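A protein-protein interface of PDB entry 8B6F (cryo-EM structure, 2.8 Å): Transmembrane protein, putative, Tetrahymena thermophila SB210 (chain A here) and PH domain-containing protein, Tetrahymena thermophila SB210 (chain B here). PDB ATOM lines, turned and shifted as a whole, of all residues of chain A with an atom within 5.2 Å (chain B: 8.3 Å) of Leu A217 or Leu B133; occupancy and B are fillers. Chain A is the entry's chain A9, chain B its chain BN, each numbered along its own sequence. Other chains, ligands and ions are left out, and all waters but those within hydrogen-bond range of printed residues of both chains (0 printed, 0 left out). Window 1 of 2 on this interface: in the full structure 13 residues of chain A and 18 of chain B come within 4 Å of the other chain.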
ATOM      1  N   ASP A 212     -31.517  -0.404 -10.869  1.00  0.00           N
ATOM      2  CA  ASP A 212     -31.385  -1.226 -12.067  1.00  0.00           C
ATOM      3  C   ASP A 212     -30.981  -2.648 -11.712  1.00  0.00           C
ATOM      4  O   ASP A 212     -31.471  -3.609 -12.314  1.00  0.00           O
ATOM      5  CB  ASP A 212     -30.367  -0.607 -13.023  1.00  0.00           C
ATOM      6  CG  ASP A 212     -30.871   0.667 -13.664  1.00  0.00           C
ATOM      7  OD1 ASP A 212     -32.039   1.033 -13.421  1.00  0.00           O
ATOM      8  OD2 ASP A 212     -30.101   1.302 -14.413  1.00  0.00           O
ATOM      9  N   TYR A 213     -30.089  -2.802 -10.734  1.00  0.00           N
ATOM     10  CA  TYR A 213     -29.709  -4.140 -10.299  1.00  0.00           C
ATOM     11  C   TYR A 213     -30.886  -4.877  -9.673  1.00  0.00           C
ATOM     12  O   TYR A 213     -31.070  -6.077  -9.907  1.00  0.00           O
ATOM     13  CB  TYR A 213     -28.551  -4.062  -9.306  1.00  0.00           C
ATOM     14  CG  TYR A 213     -28.226  -5.406  -8.722  1.00  0.00           C
ATOM     15  CD1 TYR A 213     -27.622  -6.381  -9.501  1.00  0.00           C
ATOM     16  CD2 TYR A 213     -28.541  -5.716  -7.407  1.00  0.00           C
ATOM     17  CE1 TYR A 213     -27.327  -7.616  -8.991  1.00  0.00           C
ATOM     18  CE2 TYR A 213     -28.251  -6.957  -6.884  1.00  0.00           C
ATOM     19  CZ  TYR A 213     -27.648  -7.903  -7.690  1.00  0.00           C
ATOM     20  OH  TYR A 213     -27.345  -9.144  -7.199  1.00  0.00           O
ATOM     21  N   ILE A 214     -31.696  -4.182  -8.873  1.00  0.00           N
ATOM     22  CA  ILE A 214     -32.871  -4.818  -8.284  1.00  0.00           C
ATOM     23  C   ILE A 214     -33.813  -5.298  -9.380  1.00  0.00           C
ATOM     24  O   ILE A 214     -34.367  -6.401  -9.304  1.00  0.00           O
ATOM     25  CB  ILE A 214     -33.570  -3.852  -7.309  1.00  0.00           C
ATOM     26  CG1 ILE A 214     -32.686  -3.579  -6.087  1.00  0.00           C
ATOM     27  CG2 ILE A 214     -34.925  -4.402  -6.872  1.00  0.00           C
ATOM     28  CD1 ILE A 214     -32.380  -4.795  -5.231  1.00  0.00           C
ATOM     29  N   GLN A 215     -34.019  -4.478 -10.411  1.00  0.00           N
ATOM     30  CA  GLN A 215     -34.833  -4.911 -11.541  1.00  0.00           C
ATOM     31  C   GLN A 215     -34.190  -6.096 -12.248  1.00  0.00           C
ATOM     32  O   GLN A 215     -34.875  -7.054 -12.625  1.00  0.00           O
ATOM     33  CB  GLN A 215     -35.045  -3.757 -12.520  1.00  0.00           C
ATOM     34  CG  GLN A 215     -35.865  -4.147 -13.738  1.00  0.00           C
ATOM     35  CD  GLN A 215     -36.147  -2.979 -14.653  1.00  0.00           C
ATOM     36  OE1 GLN A 215     -35.642  -1.876 -14.448  1.00  0.00           O
ATOM     37  NE2 GLN A 215     -36.962  -3.214 -15.674  1.00  0.00           N
ATOM     38  N   PHE A 216     -32.870  -6.044 -12.442  1.00  0.00           N
ATOM     39  CA  PHE A 216     -32.168  -7.119 -13.131  1.00  0.00           C
ATOM     40  C   PHE A 216     -32.308  -8.443 -12.396  1.00  0.00           C
ATOM     41  O   PHE A 216     -32.352  -9.501 -13.030  1.00  0.00           O
ATOM     42  CB  PHE A 216     -30.693  -6.744 -13.289  1.00  0.00           C
ATOM     43  CG  PHE A 216     -29.781  -7.917 -13.482  1.00  0.00           C
ATOM     44  CD1 PHE A 216     -29.611  -8.479 -14.735  1.00  0.00           C
ATOM     45  CD2 PHE A 216     -29.072  -8.441 -12.414  1.00  0.00           C
ATOM     46  CE1 PHE A 216     -28.764  -9.554 -14.916  1.00  0.00           C
ATOM     47  CE2 PHE A 216     -28.224  -9.514 -12.589  1.00  0.00           C
ATOM     48  CZ  PHE A 216     -28.070 -10.071 -13.842  1.00  0.00           C
ATOM     49  N   LEU A 217     -32.377  -8.408 -11.063  1.00  0.00           N
ATOM     50  CA  LEU A 217     -32.551  -9.640 -10.301  1.00  0.00           C
ATOM     51  C   LEU A 217     -33.756 -10.427 -10.793  1.00  0.00           C
ATOM     52  O   LEU A 217     -33.717 -11.660 -10.856  1.00  0.00           O
ATOM     53  CB  LEU A 217     -32.695  -9.319  -8.811  1.00  0.00           C
ATOM     54  CG  LEU A 217     -31.408  -8.955  -8.068  1.00  0.00           C
ATOM     55  CD1 LEU A 217     -31.721  -8.512  -6.654  1.00  0.00           C
ATOM     56  CD2 LEU A 217     -30.437 -10.124  -8.045  1.00  0.00           C
ATOM     57  N   GLY A 218     -34.824  -9.733 -11.181  1.00  0.00           N
ATOM     58  CA  GLY A 218     -36.018 -10.411 -11.652  1.00  0.00           C
ATOM     59  C   GLY A 218     -35.795 -11.253 -12.889  1.00  0.00           C
ATOM     60  O   GLY A 218     -36.627 -12.110 -13.201  1.00  0.00           O
ATOM     61  N   ASN A 219     -34.693 -11.029 -13.608  1.00  0.00           N
ATOM     62  CA  ASN A 219     -34.407 -11.843 -14.784  1.00  0.00           C
ATOM     63  C   ASN A 219     -34.205 -13.305 -14.407  1.00  0.00           C
ATOM     64  O   ASN A 219     -34.662 -14.204 -15.122  1.00  0.00           O
ATOM     65  CB  ASN A 219     -33.175 -11.305 -15.509  1.00  0.00           C
ATOM     66  CG  ASN A 219     -33.446 -10.001 -16.227  1.00  0.00           C
ATOM     67  OD1 ASN A 219     -34.473  -9.360 -16.008  1.00  0.00           O
ATOM     68  ND2 ASN A 219     -32.524  -9.600 -17.093  1.00  0.00           N
ATOM     69  N   TYR A 220     -33.519 -13.562 -13.296  1.00  0.00           N
ATOM     70  CA  TYR A 220     -33.301 -14.933 -12.856  1.00  0.00           C
ATOM     71  C   TYR A 220     -34.632 -15.637 -12.631  1.00  0.00           C
ATOM     72  O   TYR A 220     -35.544 -15.086 -12.008  1.00  0.00           O
ATOM     73  CB  TYR A 220     -32.468 -14.944 -11.575  1.00  0.00           C
ATOM     74  CG  TYR A 220     -31.052 -14.481 -11.784  1.00  0.00           C
ATOM     75  CD1 TYR A 220     -30.120 -15.300 -12.399  1.00  0.00           C
ATOM     76  CD2 TYR A 220     -30.647 -13.222 -11.369  1.00  0.00           C
ATOM     77  CE1 TYR A 220     -28.825 -14.880 -12.597  1.00  0.00           C
ATOM     78  CE2 TYR A 220     -29.355 -12.793 -11.562  1.00  0.00           C
ATOM     79  CZ  TYR A 220     -28.450 -13.624 -12.183  1.00  0.00           C
ATOM     80  OH  TYR A 220     -27.160 -13.200 -12.375  1.00  0.00           O
ATOM     81  N   VAL A 223     -35.427 -16.657  -8.661  1.00  0.00           N
ATOM     82  CA  VAL A 223     -35.905 -15.585  -7.794  1.00  0.00           C
ATOM     83  C   VAL A 223     -37.306 -15.149  -8.207  1.00  0.00           C
ATOM     84  O   VAL A 223     -38.165 -14.894  -7.355  1.00  0.00           O
ATOM     85  CB  VAL A 223     -34.921 -14.399  -7.799  1.00  0.00           C
ATOM     86  CG1 VAL A 223     -33.526 -14.850  -7.417  1.00  0.00           C
ATOM     87  CG2 VAL A 223     -34.907 -13.706  -9.139  1.00  0.00           C
ATOM     88  N   LEU B 101     -25.967 -16.215  -6.245  1.00  0.00           N
ATOM     89  CA  LEU B 101     -26.543 -14.899  -5.990  1.00  0.00           C
ATOM     90  C   LEU B 101     -25.840 -14.193  -4.837  1.00  0.00           C
ATOM     91  O   LEU B 101     -25.588 -12.984  -4.901  1.00  0.00           O
ATOM     92  CB  LEU B 101     -28.038 -15.033  -5.703  1.00  0.00           C
ATOM     93  CG  LEU B 101     -28.893 -15.532  -6.869  1.00  0.00           C
ATOM     94  CD1 LEU B 101     -30.320 -15.774  -6.415  1.00  0.00           C
ATOM     95  CD2 LEU B 101     -28.866 -14.549  -8.026  1.00  0.00           C
ATOM     96  N   ARG B 102     -25.518 -14.927  -3.769  1.00  0.00           N
ATOM     97  CA  ARG B 102     -24.857 -14.308  -2.624  1.00  0.00           C
ATOM     98  C   ARG B 102     -23.462 -13.814  -2.990  1.00  0.00           C
ATOM     99  O   ARG B 102     -23.055 -12.727  -2.568  1.00  0.00           O
ATOM    100  CB  ARG B 102     -24.797 -15.285  -1.453  1.00  0.00           C
ATOM    101  CG  ARG B 102     -24.283 -14.650  -0.170  1.00  0.00           C
ATOM    102  CD  ARG B 102     -24.914 -15.265   1.067  1.00  0.00           C
ATOM    103  NE  ARG B 102     -26.358 -15.070   1.099  1.00  0.00           N
ATOM    104  CZ  ARG B 102     -27.143 -15.436   2.103  1.00  0.00           C
ATOM    105  NH1 ARG B 102     -26.652 -16.008   3.191  1.00  0.00           N
ATOM    106  NH2 ARG B 102     -28.453 -15.229   2.012  1.00  0.00           N
ATOM    107  N   GLN B 104     -22.577 -12.879  -5.969  1.00  0.00           N
ATOM    108  CA  GLN B 104     -22.857 -11.709  -6.791  1.00  0.00           C
ATOM    109  C   GLN B 104     -23.184 -10.490  -5.939  1.00  0.00           C
ATOM    110  O   GLN B 104     -22.848  -9.362  -6.317  1.00  0.00           O
ATOM    111  CB  GLN B 104     -24.002 -12.036  -7.743  1.00  0.00           C
ATOM    112  CG  GLN B 104     -24.495 -10.887  -8.585  1.00  0.00           C
ATOM    113  CD  GLN B 104     -25.655 -11.309  -9.452  1.00  0.00           C
ATOM    114  OE1 GLN B 104     -26.716 -10.685  -9.442  1.00  0.00           O
ATOM    115  NE2 GLN B 104     -25.465 -12.387 -10.201  1.00  0.00           N
ATOM    116  N   GLN B 105     -23.834 -10.690  -4.794  1.00  0.00           N
ATOM    117  CA  GLN B 105     -24.282  -9.601  -3.937  1.00  0.00           C
ATOM    118  C   GLN B 105     -23.310  -9.297  -2.809  1.00  0.00           C
ATOM    119  O   GLN B 105     -23.634  -8.488  -1.935  1.00  0.00           O
ATOM    120  CB  GLN B 105     -25.650  -9.933  -3.341  1.00  0.00           C
ATOM    121  CG  GLN B 105     -26.737 -10.074  -4.366  1.00  0.00           C
ATOM    122  CD  GLN B 105     -28.017 -10.632  -3.789  1.00  0.00           C
ATOM    123  OE1 GLN B 105     -28.151 -10.781  -2.577  1.00  0.00           O
ATOM    124  NE2 GLN B 105     -28.970 -10.941  -4.660  1.00  0.00           N
ATOM    125  N   ALA B 106     -22.137  -9.930  -2.802  1.00  0.00           N
ATOM    126  CA  ALA B 106     -21.185  -9.774  -1.709  1.00  0.00           C
ATOM    127  C   ALA B 106     -21.086  -8.338  -1.204  1.00  0.00           C
ATOM    128  O   ALA B 106     -21.297  -8.069  -0.016  1.00  0.00           O
ATOM    129  CB  ALA B 106     -19.809 -10.272  -2.161  1.00  0.00           C
ATOM    130  N   LYS B 107     -20.757  -7.398  -2.094  1.00  0.00           N
ATOM    131  CA  LYS B 107     -20.571  -6.019  -1.655  1.00  0.00           C
ATOM    132  C   LYS B 107     -21.894  -5.374  -1.267  1.00  0.00           C
ATOM    133  O   LYS B 107     -21.948  -4.571  -0.330  1.00  0.00           O
ATOM    134  CB  LYS B 107     -19.880  -5.205  -2.747  1.00  0.00           C
ATOM    135  CG  LYS B 107     -19.107  -4.013  -2.208  1.00  0.00           C
ATOM    136  CD  LYS B 107     -18.518  -3.171  -3.326  1.00  0.00           C
ATOM    137  CE  LYS B 107     -19.464  -2.063  -3.757  1.00  0.00           C
ATOM    138  NZ  LYS B 107     -19.600  -1.013  -2.711  1.00  0.00           N
ATOM    139  N   PHE B 108     -22.972  -5.697  -1.984  1.00  0.00           N
ATOM    140  CA  PHE B 108     -24.275  -5.145  -1.631  1.00  0.00           C
ATOM    141  C   PHE B 108     -24.697  -5.554  -0.227  1.00  0.00           C
ATOM    142  O   PHE B 108     -25.424  -4.812   0.442  1.00  0.00           O
ATOM    143  CB  PHE B 108     -25.324  -5.584  -2.652  1.00  0.00           C
ATOM    144  CG  PHE B 108     -25.031  -5.137  -4.057  1.00  0.00           C
ATOM    145  CD1 PHE B 108     -24.338  -3.960  -4.301  1.00  0.00           C
ATOM    146  CD2 PHE B 108     -25.451  -5.896  -5.136  1.00  0.00           C
ATOM    147  CE1 PHE B 108     -24.071  -3.552  -5.593  1.00  0.00           C
ATOM    148  CE2 PHE B 108     -25.186  -5.493  -6.430  1.00  0.00           C
ATOM    149  CZ  PHE B 108     -24.494  -4.319  -6.659  1.00  0.00           C
ATOM    150  N   ILE B 109     -24.253  -6.723   0.239  1.00  0.00           N
ATOM    151  CA  ILE B 109     -24.585  -7.154   1.593  1.00  0.00           C
ATOM    152  C   ILE B 109     -23.991  -6.194   2.614  1.00  0.00           C
ATOM    153  O   ILE B 109     -24.667  -5.763   3.553  1.00  0.00           O
ATOM    154  CB  ILE B 109     -24.109  -8.600   1.833  1.00  0.00           C
ATOM    155  CG1 ILE B 109     -24.815  -9.578   0.886  1.00  0.00           C
ATOM    156  CG2 ILE B 109     -24.341  -9.011   3.286  1.00  0.00           C
ATOM    157  CD1 ILE B 109     -26.317  -9.656   1.054  1.00  0.00           C
ATOM    158  N   GLN B 110     -22.713  -5.844   2.450  1.00  0.00           N
ATOM    159  CA  GLN B 110     -22.097  -4.926   3.402  1.00  0.00           C
ATOM    160  C   GLN B 110     -22.674  -3.524   3.274  1.00  0.00           C
ATOM    161  O   GLN B 110     -22.812  -2.820   4.279  1.00  0.00           O
ATOM    162  CB  GLN B 110     -20.577  -4.905   3.221  1.00  0.00           C
ATOM    163  CG  GLN B 110     -20.092  -4.369   1.886  1.00  0.00           C
ATOM    164  CD  GLN B 110     -18.612  -4.053   1.899  1.00  0.00           C
ATOM    165  OE1 GLN B 110     -17.903  -4.387   2.846  1.00  0.00           O
ATOM    166  NE2 GLN B 110     -18.137  -3.404   0.841  1.00  0.00           N
ATOM    167  N   LEU B 111     -23.017  -3.099   2.056  1.00  0.00           N
ATOM    168  CA  LEU B 111     -23.671  -1.805   1.892  1.00  0.00           C
ATOM    169  C   LEU B 111     -25.000  -1.776   2.633  1.00  0.00           C
ATOM    170  O   LEU B 111     -25.324  -0.794   3.309  1.00  0.00           O
ATOM    171  CB  LEU B 111     -23.876  -1.502   0.409  1.00  0.00           C
ATOM    172  CG  LEU B 111     -22.622  -1.156  -0.397  1.00  0.00           C
ATOM    173  CD1 LEU B 111     -22.962  -1.051  -1.873  1.00  0.00           C
ATOM    174  CD2 LEU B 111     -21.992   0.134   0.095  1.00  0.00           C
ATOM    175  N   GLU B 112     -25.783  -2.851   2.517  1.00  0.00           N
ATOM    176  CA  GLU B 112     -27.054  -2.919   3.228  1.00  0.00           C
ATOM    177  C   GLU B 112     -26.839  -2.934   4.734  1.00  0.00           C
ATOM    178  O   GLU B 112     -27.598  -2.310   5.483  1.00  0.00           O
ATOM    179  CB  GLU B 112     -27.829  -4.160   2.783  1.00  0.00           C
ATOM    180  CG  GLU B 112     -29.209  -4.287   3.407  1.00  0.00           C
ATOM    181  CD  GLU B 112     -29.917  -5.560   2.987  1.00  0.00           C
ATOM    182  OE1 GLU B 112     -29.302  -6.369   2.262  1.00  0.00           O
ATOM    183  OE2 GLU B 112     -31.086  -5.752   3.382  1.00  0.00           O
ATOM    184  N   ILE B 116     -28.318  -0.197   7.323  1.00  0.00           N
ATOM    185  CA  ILE B 116     -29.127  -0.536   8.489  1.00  0.00           C
ATOM    186  C   ILE B 116     -28.525   0.070   9.750  1.00  0.00           C
ATOM    187  O   ILE B 116     -29.244   0.607  10.600  1.00  0.00           O
ATOM    188  CB  ILE B 116     -29.274  -2.064   8.608  1.00  0.00           C
ATOM    189  CG1 ILE B 116     -30.086  -2.609   7.432  1.00  0.00           C
ATOM    190  CG2 ILE B 116     -29.942  -2.441   9.926  1.00  0.00           C
ATOM    191  CD1 ILE B 116     -30.057  -4.116   7.310  1.00  0.00           C
ATOM    192  N   THR B 128     -28.153   4.110  -0.862  1.00  0.00           N
ATOM    193  CA  THR B 128     -28.200   2.657  -0.782  1.00  0.00           C
ATOM    194  C   THR B 128     -29.558   2.137  -0.335  1.00  0.00           C
ATOM    195  O   THR B 128     -29.688   0.942  -0.053  1.00  0.00           O
ATOM    196  CB  THR B 128     -27.115   2.149   0.170  1.00  0.00           C
ATOM    197  OG1 THR B 128     -27.264   2.773   1.452  1.00  0.00           O
ATOM    198  CG2 THR B 128     -25.732   2.453  -0.382  1.00  0.00           C
ATOM    199  N   SER B 129     -30.569   2.999  -0.259  1.00  0.00           N
ATOM    200  CA  SER B 129     -31.884   2.549   0.187  1.00  0.00           C
ATOM    201  C   SER B 129     -32.444   1.412  -0.659  1.00  0.00           C
ATOM    202  O   SER B 129     -33.036   0.486  -0.076  1.00  0.00           O
ATOM    203  CB  SER B 129     -32.857   3.736   0.222  1.00  0.00           C
ATOM    204  OG  SER B 129     -32.907   4.416  -1.018  1.00  0.00           O
ATOM    205  N   PRO B 130     -32.312   1.402  -1.988  1.00  0.00           N
ATOM    206  CA  PRO B 130     -32.922   0.311  -2.767  1.00  0.00           C
ATOM    207  C   PRO B 130     -32.384  -1.066  -2.416  1.00  0.00           C
ATOM    208  O   PRO B 130     -33.072  -2.062  -2.665  1.00  0.00           O
ATOM    209  CB  PRO B 130     -32.592   0.686  -4.220  1.00  0.00           C
ATOM    210  CG  PRO B 130     -32.238   2.127  -4.187  1.00  0.00           C
ATOM    211  CD  PRO B 130     -31.597   2.349  -2.861  1.00  0.00           C
ATOM    212  N   LEU B 131     -31.182  -1.157  -1.848  1.00  0.00           N
ATOM    213  CA  LEU B 131     -30.537  -2.444  -1.588  1.00  0.00           C
ATOM    214  C   LEU B 131     -31.196  -3.106  -0.382  1.00  0.00           C
ATOM    215  O   LEU B 131     -30.738  -3.011   0.759  1.00  0.00           O
ATOM    216  CB  LEU B 131     -29.040  -2.258  -1.375  1.00  0.00           C
ATOM    217  CG  LEU B 131     -28.239  -1.808  -2.598  1.00  0.00           C
ATOM    218  CD1 LEU B 131     -26.804  -1.513  -2.211  1.00  0.00           C
ATOM    219  CD2 LEU B 131     -28.287  -2.856  -3.698  1.00  0.00           C
ATOM    220  N   VAL B 132     -32.300  -3.790  -0.650  1.00  0.00           N
ATOM    221  CA  VAL B 132     -32.985  -4.621   0.338  1.00  0.00           C
ATOM    222  C   VAL B 132     -33.052  -6.020  -0.264  1.00  0.00           C
ATOM    223  O   VAL B 132     -33.968  -6.352  -1.019  1.00  0.00           O
ATOM    224  CB  VAL B 132     -34.373  -4.087   0.696  1.00  0.00           C
ATOM    225  CG1 VAL B 132     -35.021  -4.955   1.762  1.00  0.00           C
ATOM    226  CG2 VAL B 132     -34.269  -2.652   1.176  1.00  0.00           C
ATOM    227  N   LEU B 133     -32.075  -6.852   0.078  1.00  0.00           N
ATOM    228  CA  LEU B 133     -31.899  -8.159  -0.536  1.00  0.00           C
ATOM    229  C   LEU B 133     -32.363  -9.256   0.412  1.00  0.00           C
ATOM    230  O   LEU B 133     -32.149  -9.177   1.624  1.00  0.00           O
ATOM    231  CB  LEU B 133     -30.432  -8.380  -0.906  1.00  0.00           C
ATOM    232  CG  LEU B 133     -29.788  -7.265  -1.731  1.00  0.00           C
ATOM    233  CD1 LEU B 133     -28.289  -7.473  -1.828  1.00  0.00           C
ATOM    234  CD2 LEU B 133     -30.407  -7.192  -3.116  1.00  0.00           C
ATOM    235  N   TRP B 134     -33.005 -10.282  -0.153  1.00  0.00           N
ATOM    236  CA  TRP B 134     -33.473 -11.427   0.615  1.00  0.00           C
ATOM    237  C   TRP B 134     -32.953 -12.750   0.066  1.00  0.00           C
ATOM    238  O   TRP B 134     -33.374 -13.810   0.542  1.00  0.00           O
ATOM    239  CB  TRP B 134     -35.005 -11.455   0.652  1.00  0.00           C
ATOM    240  CG  TRP B 134     -35.625 -11.493  -0.706  1.00  0.00           C
ATOM    241  CD1 TRP B 134     -35.988 -10.423  -1.467  1.00  0.00           C
ATOM    242  CD2 TRP B 134     -35.954 -12.660  -1.468  1.00  0.00           C
ATOM    243  NE1 TRP B 134     -36.522 -10.851  -2.658  1.00  0.00           N
ATOM    244  CE2 TRP B 134     -36.512 -12.220  -2.683  1.00  0.00           C
ATOM    245  CE3 TRP B 134     -35.829 -14.033  -1.241  1.00  0.00           C
ATOM    246  CZ2 TRP B 134     -36.946 -13.103  -3.668  1.00  0.00           C
ATOM    247  CZ3 TRP B 134     -36.259 -14.910  -2.221  1.00  0.00           C
ATOM    248  CH2 TRP B 134     -36.811 -14.441  -3.421  1.00  0.00           C
ATOM    249  N   ASN B 135     -32.055 -12.722  -0.913  1.00  0.00           N
ATOM    250  CA  ASN B 135     -31.515 -13.948  -1.491  1.00  0.00           C
ATOM    251  C   ASN B 135     -30.173 -13.693  -2.169  1.00  0.00           C
ATOM    252  O   ASN B 135     -29.939 -12.624  -2.728  1.00  0.00           O
ATOM    253  CB  ASN B 135     -32.498 -14.543  -2.497  1.00  0.00           C
ATOM    254  CG  ASN B 135     -32.878 -13.562  -3.587  1.00  0.00           C
ATOM    255  OD1 ASN B 135     -32.265 -12.506  -3.730  1.00  0.00           O
ATOM    256  ND2 ASN B 135     -33.893 -13.911  -4.366  1.00  0.00           N
ATOM    257  OXT ASN B 135     -29.295 -14.556  -2.183  1.00  0.00           O
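Of the printed residues of chain A, Leu B133 touches Ile A214 (3.8 Å) and Leu A217 (3.998 Å).
No residue of chain B comes within 4 Å of Gly A218.
Of the printed residues of chain A, Pro B130 touches Ile A214.
Of the printed residues of chain A, Gln B104 touches Tyr A213 (2.8 Å), Phe A216 (3.7 Å) and Tyr A220 (2.9 Å).
Of the printed residues of chain B, Ile A214 touches Pro B130 and Leu B133.
Of the printed residues of chain A, Gln B105 touches Tyr A213 and Leu A217.
Asp A212 touches none of the printed residues of chain B.
Thr B128 touches none of the printed residues of chain A.
The nearest printed residue of chain B that does not touch Leu A217 is Gln B104 (4.01 Å).
The nearest printed residue of chain A that does not touch Leu B133 is Tyr A213 (4.3 Å).
The nearest printed residue of chain B that does not touch Phe A216 is Leu B101 (6.8 Å).
The side-chain amide oxygen of Gln B105 sits close to the chain-end carboxylate of Asn B135 (2.6 Å).
Tyr A213 touches Gln B105.
CE2 of Tyr A213 touches CE2 of Phe B108 (3.4 Å).
Pro B130 touches Ile A214 (O to CG1, 3.8 Å).
Ile A214 touches Leu B133.
OE1 of Gln B104 touches CE2 of Phe A216 (3.7 Å).
Leu A217 touches Gln B105.
Leu A217 touches Leu B133.
Leu B101 touches Tyr A220 (CD2 to CE2, 3.98 Å).
Leu B101 touches Val A223 (CD1 to CG1, 3.5 Å).
Asn B135 touches Val A223.
Printed residues of chain B that touch a printed residue of chain A: Leu B101, Gln B104, Gln B105, Phe B108, Pro B130, Leu B133 and Asn B135.
Hydrophobic or aromatic side chains of chain B that line the printed part of chain A: Leu B101, Phe B108 and Leu B133.
Along chain B the printed residues that touch a printed residue of chain A span positions 101 to 135.
Of the 10 printed residues of chain A, 6 touch a printed residue of chain B.
Printed residues of chain A that touch a printed residue of chain B: Tyr A213, Ile A214, Phe A216, Leu A217, Tyr A220 and Val A223.
Among the printed residues, 12 pairs touch across the chains.
Among the printed residues, no Asp or Glu carboxylate lies within 4 Å of a Lys or Arg side-chain nitrogen of the other chain.
The side-chain hydroxyl (OH) of Tyr A213 lies within hydrogen-bond range of the side-chain amide oxygen (OE1) of Gln B104.
OH of Tyr A220 sits at hydrogen-bond distance from NE2 of Gln B104 (2.9 Å).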
